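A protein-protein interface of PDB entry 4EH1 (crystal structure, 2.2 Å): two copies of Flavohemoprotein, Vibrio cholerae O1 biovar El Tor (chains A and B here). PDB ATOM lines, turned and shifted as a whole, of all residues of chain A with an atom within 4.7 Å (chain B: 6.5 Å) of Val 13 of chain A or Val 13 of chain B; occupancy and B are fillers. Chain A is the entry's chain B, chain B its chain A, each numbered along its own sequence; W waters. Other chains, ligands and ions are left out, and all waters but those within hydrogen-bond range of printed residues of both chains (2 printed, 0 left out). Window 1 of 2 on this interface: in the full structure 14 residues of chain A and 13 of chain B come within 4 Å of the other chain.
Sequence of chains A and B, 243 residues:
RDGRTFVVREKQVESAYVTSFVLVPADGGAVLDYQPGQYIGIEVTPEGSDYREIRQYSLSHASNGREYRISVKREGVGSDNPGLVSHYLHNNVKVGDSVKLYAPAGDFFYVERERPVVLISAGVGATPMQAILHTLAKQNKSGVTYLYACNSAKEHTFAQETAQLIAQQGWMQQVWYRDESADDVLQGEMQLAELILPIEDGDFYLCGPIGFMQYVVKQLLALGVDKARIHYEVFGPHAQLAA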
ATOM      1  N   LYS A  11      17.263 -28.212 -29.542  1.00  0.00           N
ATOM      2  CA  LYS A  11      17.027 -29.290 -28.617  1.00  0.00           C
ATOM      3  C   LYS A  11      15.628 -29.032 -28.048  1.00  0.00           C
ATOM      4  O   LYS A  11      15.413 -28.147 -27.206  1.00  0.00           O
ATOM      5  CB  LYS A  11      18.149 -29.341 -27.583  1.00  0.00           C
ATOM      6  CG  LYS A  11      17.988 -30.362 -26.474  1.00  0.00           C
ATOM      7  CD  LYS A  11      19.313 -30.455 -25.684  1.00  0.00           C
ATOM      8  CE  LYS A  11      19.236 -31.408 -24.489  1.00  0.00           C
ATOM      9  NZ  LYS A  11      20.470 -31.311 -23.619  1.00  0.00           N
ATOM     10  N   GLN A  12      14.673 -29.784 -28.589  1.00  0.00           N
ATOM     11  CA  GLN A  12      13.250 -29.619 -28.331  1.00  0.00           C
ATOM     12  C   GLN A  12      12.784 -30.729 -27.405  1.00  0.00           C
ATOM     13  O   GLN A  12      13.082 -31.896 -27.639  1.00  0.00           O
ATOM     14  CB  GLN A  12      12.465 -29.761 -29.638  1.00  0.00           C
ATOM     15  CG  GLN A  12      11.835 -28.487 -30.177  1.00  0.00           C
ATOM     16  CD  GLN A  12      10.357 -28.329 -29.814  1.00  0.00           C
ATOM     17  OE1 GLN A  12       9.804 -27.222 -29.904  1.00  0.00           O
ATOM     18  NE2 GLN A  12       9.711 -29.439 -29.410  1.00  0.00           N
ATOM     19  N   VAL A  13      12.033 -30.369 -26.373  1.00  0.00           N
ATOM     20  CA  VAL A  13      11.347 -31.358 -25.549  1.00  0.00           C
ATOM     21  C   VAL A  13      10.082 -31.834 -26.268  1.00  0.00           C
ATOM     22  O   VAL A  13       9.220 -31.028 -26.627  1.00  0.00           O
ATOM     23  CB  VAL A  13      10.937 -30.760 -24.193  1.00  0.00           C
ATOM     24  CG1 VAL A  13      10.236 -31.829 -23.299  1.00  0.00           C
ATOM     25  CG2 VAL A  13      12.139 -30.165 -23.499  1.00  0.00           C
ATOM     26  N   GLU A  14       9.965 -33.141 -26.469  1.00  0.00           N
ATOM     27  CA  GLU A  14       8.784 -33.682 -27.129  1.00  0.00           C
ATOM     28  C   GLU A  14       7.802 -34.179 -26.103  1.00  0.00           C
ATOM     29  O   GLU A  14       6.608 -34.012 -26.257  1.00  0.00           O
ATOM     30  CB  GLU A  14       9.142 -34.809 -28.082  1.00  0.00           C
ATOM     31  CG  GLU A  14      10.182 -34.416 -29.111  1.00  0.00           C
ATOM     32  CD  GLU A  14       9.653 -33.414 -30.133  1.00  0.00           C
ATOM     33  OE1 GLU A  14       8.439 -33.099 -30.087  1.00  0.00           O
ATOM     34  OE2 GLU A  14      10.442 -32.965 -31.012  1.00  0.00           O
ATOM     35  N   SER A  15       8.300 -34.792 -25.040  1.00  0.00           N
ATOM     36  CA  SER A  15       7.391 -35.167 -23.965  1.00  0.00           C
ATOM     37  C   SER A  15       8.181 -35.279 -22.680  1.00  0.00           C
ATOM     38  O   SER A  15       9.354 -34.867 -22.643  1.00  0.00           O
ATOM     39  CB  SER A  15       6.679 -36.479 -24.304  1.00  0.00           C
ATOM     40  OG  SER A  15       7.629 -37.471 -24.628  1.00  0.00           O
ATOM     41  N   VAL A  18      11.125 -37.656 -23.486  1.00  0.00           N
ATOM     42  CA  VAL A  18      11.700 -37.641 -24.842  1.00  0.00           C
ATOM     43  C   VAL A  18      12.132 -36.230 -25.290  1.00  0.00           C
ATOM     44  O   VAL A  18      11.354 -35.279 -25.238  1.00  0.00           O
ATOM     45  CB  VAL A  18      10.683 -38.202 -25.853  1.00  0.00           C
ATOM     46  CG1 VAL A  18      11.208 -38.062 -27.269  1.00  0.00           C
ATOM     47  CG2 VAL A  18      10.333 -39.663 -25.489  1.00  0.00           C
ATOM     48  N   THR A  19      13.367 -36.098 -25.733  1.00  0.00           N
ATOM     49  CA  THR A  19      13.835 -34.806 -26.210  1.00  0.00           C
ATOM     50  C   THR A  19      14.457 -34.969 -27.590  1.00  0.00           C
ATOM     51  O   THR A  19      15.148 -35.943 -27.822  1.00  0.00           O
ATOM     52  CB  THR A  19      14.852 -34.201 -25.228  1.00  0.00           C
ATOM     53  OG1 THR A  19      14.149 -33.698 -24.080  1.00  0.00           O
ATOM     54  CG2 THR A  19      15.640 -33.045 -25.894  1.00  0.00           C
ATOM     55  N   VAL A  95      22.529 -27.233 -27.050  1.00  0.00           N
ATOM     56  CA  VAL A  95      22.606 -26.497 -28.307  1.00  0.00           C
ATOM     57  C   VAL A  95      24.007 -25.876 -28.394  1.00  0.00           C
ATOM     58  O   VAL A  95      24.503 -25.309 -27.414  1.00  0.00           O
ATOM     59  CB  VAL A  95      21.540 -25.382 -28.377  1.00  0.00           C
ATOM     60  CG1 VAL A  95      21.775 -24.407 -29.648  1.00  0.00           C
ATOM     61  CG2 VAL A  95      20.100 -26.001 -28.371  1.00  0.00           C
ATOM     62  N   LYS B  11       9.321 -25.564 -27.038  1.00  0.00           N
ATOM     63  CA  LYS B  11       9.859 -25.975 -25.748  1.00  0.00           C
ATOM     64  C   LYS B  11      11.312 -26.413 -25.962  1.00  0.00           C
ATOM     65  O   LYS B  11      11.573 -27.524 -26.384  1.00  0.00           O
ATOM     66  CB  LYS B  11       9.029 -27.134 -25.198  1.00  0.00           C
ATOM     67  CG  LYS B  11       9.179 -27.352 -23.710  1.00  0.00           C
ATOM     68  CD  LYS B  11       8.204 -28.410 -23.174  1.00  0.00           C
ATOM     69  CE  LYS B  11       8.531 -28.711 -21.701  1.00  0.00           C
ATOM     70  NZ  LYS B  11       7.640 -29.749 -21.160  1.00  0.00           N
ATOM     71  N   GLN B  12      12.246 -25.505 -25.722  1.00  0.00           N
ATOM     72  CA  GLN B  12      13.649 -25.770 -25.999  1.00  0.00           C
ATOM     73  C   GLN B  12      14.439 -25.934 -24.706  1.00  0.00           C
ATOM     74  O   GLN B  12      14.268 -25.168 -23.760  1.00  0.00           O
ATOM     75  CB  GLN B  12      14.279 -24.638 -26.824  1.00  0.00           C
ATOM     76  CG  GLN B  12      13.735 -24.504 -28.248  1.00  0.00           C
ATOM     77  CD  GLN B  12      14.432 -25.414 -29.256  1.00  0.00           C
ATOM     78  OE1 GLN B  12      15.670 -25.559 -29.263  1.00  0.00           O
ATOM     79  NE2 GLN B  12      13.638 -26.024 -30.123  1.00  0.00           N
ATOM     80  N   VAL B  13      15.307 -26.937 -24.686  1.00  0.00           N
ATOM     81  CA  VAL B  13      16.204 -27.131 -23.565  1.00  0.00           C
ATOM     82  C   VAL B  13      17.328 -26.135 -23.665  1.00  0.00           C
ATOM     83  O   VAL B  13      18.024 -26.087 -24.655  1.00  0.00           O
ATOM     84  CB  VAL B  13      16.772 -28.554 -23.543  1.00  0.00           C
ATOM     85  CG1 VAL B  13      17.728 -28.741 -22.355  1.00  0.00           C
ATOM     86  CG2 VAL B  13      15.630 -29.535 -23.460  1.00  0.00           C
ATOM     87  N   GLU B  14      17.501 -25.327 -22.632  1.00  0.00           N
ATOM     88  CA  GLU B  14      18.595 -24.374 -22.623  1.00  0.00           C
ATOM     89  C   GLU B  14      19.833 -24.907 -21.901  1.00  0.00           C
ATOM     90  O   GLU B  14      20.935 -24.570 -22.273  1.00  0.00           O
ATOM     91  CB  GLU B  14      18.169 -23.052 -21.974  1.00  0.00           C
ATOM     92  CG  GLU B  14      16.997 -22.385 -22.638  1.00  0.00           C
ATOM     93  CD  GLU B  14      17.330 -21.896 -24.066  1.00  0.00           C
ATOM     94  OE1 GLU B  14      18.488 -22.074 -24.526  1.00  0.00           O
ATOM     95  OE2 GLU B  14      16.430 -21.307 -24.722  1.00  0.00           O
ATOM     96  N   SER B  15      19.645 -25.689 -20.843  1.00  0.00           N
ATOM     97  CA  SER B  15      20.779 -26.256 -20.094  1.00  0.00           C
ATOM     98  C   SER B  15      20.201 -27.362 -19.246  1.00  0.00           C
ATOM     99  O   SER B  15      19.018 -27.650 -19.397  1.00  0.00           O
ATOM    100  CB  SER B  15      21.507 -25.206 -19.242  1.00  0.00           C
ATOM    101  OG  SER B  15      20.632 -24.485 -18.398  1.00  0.00           O
ATOM    102  N   ALA B  16      21.018 -28.010 -18.412  1.00  0.00           N
ATOM    103  CA  ALA B  16      20.561 -29.171 -17.627  1.00  0.00           C
ATOM    104  C   ALA B  16      19.228 -28.930 -16.908  1.00  0.00           C
ATOM    105  O   ALA B  16      18.377 -29.782 -16.879  1.00  0.00           O
ATOM    106  CB  ALA B  16      21.616 -29.600 -16.614  1.00  0.00           C
ATOM    107  N   TYR B  17      19.028 -27.764 -16.328  1.00  0.00           N
ATOM    108  CA  TYR B  17      17.808 -27.587 -15.543  1.00  0.00           C
ATOM    109  C   TYR B  17      16.872 -26.484 -16.081  1.00  0.00           C
ATOM    110  O   TYR B  17      15.786 -26.253 -15.539  1.00  0.00           O
ATOM    111  CB  TYR B  17      18.190 -27.296 -14.110  1.00  0.00           C
ATOM    112  CG  TYR B  17      19.094 -28.373 -13.533  1.00  0.00           C
ATOM    113  CD1 TYR B  17      18.634 -29.670 -13.362  1.00  0.00           C
ATOM    114  CD2 TYR B  17      20.397 -28.081 -13.163  1.00  0.00           C
ATOM    115  CE1 TYR B  17      19.439 -30.666 -12.841  1.00  0.00           C
ATOM    116  CE2 TYR B  17      21.215 -29.063 -12.607  1.00  0.00           C
ATOM    117  CZ  TYR B  17      20.727 -30.349 -12.453  1.00  0.00           C
ATOM    118  OH  TYR B  17      21.542 -31.308 -11.935  1.00  0.00           O
ATOM    119  N   VAL B  18      17.293 -25.819 -17.146  1.00  0.00           N
ATOM    120  CA  VAL B  18      16.521 -24.709 -17.673  1.00  0.00           C
ATOM    121  C   VAL B  18      15.959 -25.056 -19.060  1.00  0.00           C
ATOM    122  O   VAL B  18      16.684 -25.491 -19.982  1.00  0.00           O
ATOM    123  CB  VAL B  18      17.363 -23.443 -17.786  1.00  0.00           C
ATOM    124  CG1 VAL B  18      16.553 -22.324 -18.490  1.00  0.00           C
ATOM    125  CG2 VAL B  18      17.887 -22.986 -16.407  1.00  0.00           C
ATOM    126  N   THR B  19      14.665 -24.852 -19.185  1.00  0.00           N
ATOM    127  CA  THR B  19      13.948 -25.084 -20.426  1.00  0.00           C
ATOM    128  C   THR B  19      13.151 -23.831 -20.807  1.00  0.00           C
ATOM    129  O   THR B  19      12.502 -23.222 -19.950  1.00  0.00           O
ATOM    130  CB  THR B  19      13.042 -26.333 -20.275  1.00  0.00           C
ATOM    131  OG1 THR B  19      13.885 -27.500 -20.323  1.00  0.00           O
ATOM    132  CG2 THR B  19      11.965 -26.414 -21.425  1.00  0.00           C
ATOM    133  N   SER B  20      13.235 -23.418 -22.077  1.00  0.00           N
ATOM    134  CA  SER B  20      12.492 -22.243 -22.542  1.00  0.00           C
ATOM    135  C   SER B  20      11.110 -22.640 -23.091  1.00  0.00           C
ATOM    136  O   SER B  20      10.939 -23.734 -23.624  1.00  0.00           O
ATOM    137  CB  SER B  20      13.245 -21.497 -23.657  1.00  0.00           C
ATOM    138  OG  SER B  20      14.230 -20.632 -23.164  1.00  0.00           O
ATOM    139  N   HIS B  90       8.015 -28.137 -16.857  1.00  0.00           N
ATOM    140  CA  HIS B  90       8.980 -29.072 -17.432  1.00  0.00           C
ATOM    141  C   HIS B  90       8.336 -30.432 -17.773  1.00  0.00           C
ATOM    142  O   HIS B  90       8.457 -30.913 -18.890  1.00  0.00           O
ATOM    143  CB  HIS B  90      10.181 -29.300 -16.478  1.00  0.00           C
ATOM    144  CG  HIS B  90      11.238 -28.244 -16.564  1.00  0.00           C
ATOM    145  ND1 HIS B  90      12.508 -28.501 -17.037  1.00  0.00           N
ATOM    146  CD2 HIS B  90      11.217 -26.921 -16.248  1.00  0.00           C
ATOM    147  CE1 HIS B  90      13.225 -27.390 -17.015  1.00  0.00           C
ATOM    148  NE2 HIS B  90      12.467 -26.416 -16.538  1.00  0.00           N
ATOM    149  N   VAL B  93       3.657 -29.740 -19.257  1.00  0.00           N
ATOM    150  CA  VAL B  93       3.162 -28.793 -20.234  1.00  0.00           C
ATOM    151  C   VAL B  93       3.906 -28.946 -21.571  1.00  0.00           C
ATOM    152  O   VAL B  93       5.019 -28.451 -21.723  1.00  0.00           O
ATOM    153  CB  VAL B  93       3.266 -27.365 -19.699  1.00  0.00           C
ATOM    154  CG1 VAL B  93       2.793 -26.365 -20.771  1.00  0.00           C
ATOM    155  CG2 VAL B  93       2.470 -27.239 -18.379  1.00  0.00           C
ATOM    156  N   LYS B  94       3.272 -29.621 -22.529  1.00  0.00           N
ATOM    157  CA  LYS B  94       3.885 -29.898 -23.831  1.00  0.00           C
ATOM    158  C   LYS B  94       3.653 -28.807 -24.872  1.00  0.00           C
ATOM    159  O   LYS B  94       2.766 -27.960 -24.714  1.00  0.00           O
ATOM    160  CB  LYS B  94       3.317 -31.205 -24.408  1.00  0.00           C
ATOM    161  CG  LYS B  94       3.247 -32.351 -23.420  1.00  0.00           C
ATOM    162  CD  LYS B  94       2.897 -33.674 -24.102  1.00  0.00           C
ATOM    163  CE  LYS B  94       1.449 -33.657 -24.606  1.00  0.00           C
ATOM    164  NZ  LYS B  94       0.511 -32.969 -23.646  1.00  0.00           N
ATOM    165  N   VAL B  95       4.451 -28.846 -25.948  1.00  0.00           N
ATOM    166  CA  VAL B  95       4.128 -28.102 -27.155  1.00  0.00           C
ATOM    167  C   VAL B  95       2.693 -28.410 -27.578  1.00  0.00           C
ATOM    168  O   VAL B  95       2.314 -29.579 -27.720  1.00  0.00           O
ATOM    169  CB  VAL B  95       5.073 -28.456 -28.327  1.00  0.00           C
ATOM    170  CG1 VAL B  95       4.625 -27.749 -29.605  1.00  0.00           C
ATOM    171  CG2 VAL B  95       6.520 -28.076 -27.987  1.00  0.00           C
HETATM  172  O   HOH W   1      20.778 -26.328 -24.645  1.00  0.00           O
HETATM  173  O   HOH W   2       6.497 -30.919 -25.805  1.00  0.00           O
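The side-chain amide oxygen (OE1) of Gln 12 of chain A lies within hydrogen-bond range of the backbone NH (N) of Lys 11 of chain B (3.3 Å). O of Lys 11 of chain B is in hydrogen-bond range of N of Val 13 of chain A (2.9 Å). OE1 of Gln 12 of chain B is in hydrogen-bond range of N of Lys 11 of chain A (3.1 Å). The backbone carbonyl oxygen (O) of Lys 11 of chain A sits at hydrogen-bond distance from the backbone NH (N) of Val 13 of chain B, 2.8 Å away.
The side-chain amino group of Lys 11 of chain B sits at hydrogen-bond distance from the backbone carbonyl oxygen of His 90 of chain B, 2.7 Å away. The side-chain amino group (NZ) of Lys 11 of chain B lies within hydrogen-bond range of the backbone carbonyl oxygen (O) of Val 93 of chain B (3.0 Å). The backbone carbonyl oxygen of Gln 12 of chain B lies within hydrogen-bond range of the backbone NH of Ser 20 of chain B, 2.6 Å away.
Lys 11 of chain A touches Lys 11 of chain B. Gln 12 of chain A touches Gln 12 of chain B. NE2 of Gln 12 of chain A touches CG2 of Val 95 of chain B, 3.8 Å away. CG2 of Val 13 of chain A touches CG2 of Val 13 of chain B, at 3.5 Å.
Of the printed residues of chain B, Lys 11 of chain A touches Lys 11 (3.98 Å), Gln 12 (3.1 Å) and Val 13 (2.8 Å). Printed residues of chain B within 4 Å of Gln 12 of chain A: Lys 11 (3.3 Å), Gln 12 (3.1 Å) and Val 95 (3.8 Å). Val 13 of chain A touches just these residues of chain B: Lys 11 and Val 13. Ser 15 of chain A touches none of the printed residues of chain B. Of the printed residues of chain A, Lys 11 of chain B touches Lys 11 (3.98 Å), Gln 12 (3.3 Å) and Val 13 (2.9 Å). Printed residues of chain A within 4 Å of Gln 12 of chain B: Lys 11 and Gln 12. Val 13 of chain B touches just these residues of chain A: Lys 11 (2.8 Å) and Val 13 (3.5 Å). Thr 19 of chain B touches none of the printed residues of chain A. Printed residues of chain A within 4 Å of Val 95 of chain B: Gln 12 (3.8 Å). The nearest residue of chain B that does not touch Val 13 of chain A is Val 95 of chain B (4.2 Å).
Of the 8 printed residues of chain A, 3 touch a printed residue of chain B. Of the 14 printed residues of chain B, 4 touch a printed residue of chain A. Printed residues of chain B that touch a printed residue of chain A: Lys 11, Gln 12, Val 13 and Val 95. Hydrophobic or aromatic side chains of chain B that line the printed part of chain A: Val 13 and Val 95. Among the printed residues, no Asp or Glu carboxylate lies within 4 Å of a Lys or Arg side-chain nitrogen of the other chain.
Lys 11 of chain A touches its own counterpart, Lys 11 of chain B. Lys 11 of chain A touches Gln 12 of chain B, and with the chains exchanged Gln 12 of chain A touches Lys 11 of chain B. Lys 11 of chain A touches Val 13 of chain B, and with the chains exchanged Val 13 of chain A touches Lys 11 of chain B. Val 13 of chain A touches its own counterpart, Val 13 of chain B. 8 positions are printed for both chains.
Water W1 lies within hydrogen-bond range of O of Val 13 of chain B (2.8 Å), O of Glu 14 of chain B (3.0 Å) and N of Val 95 of chain A (3.1 Å). Water W2 lies within hydrogen-bond range of O of Val 13 of chain A (2.8 Å), N of Val 95 of chain B (2.9 Å) and O of Glu 14 of chain A (3.1 Å).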
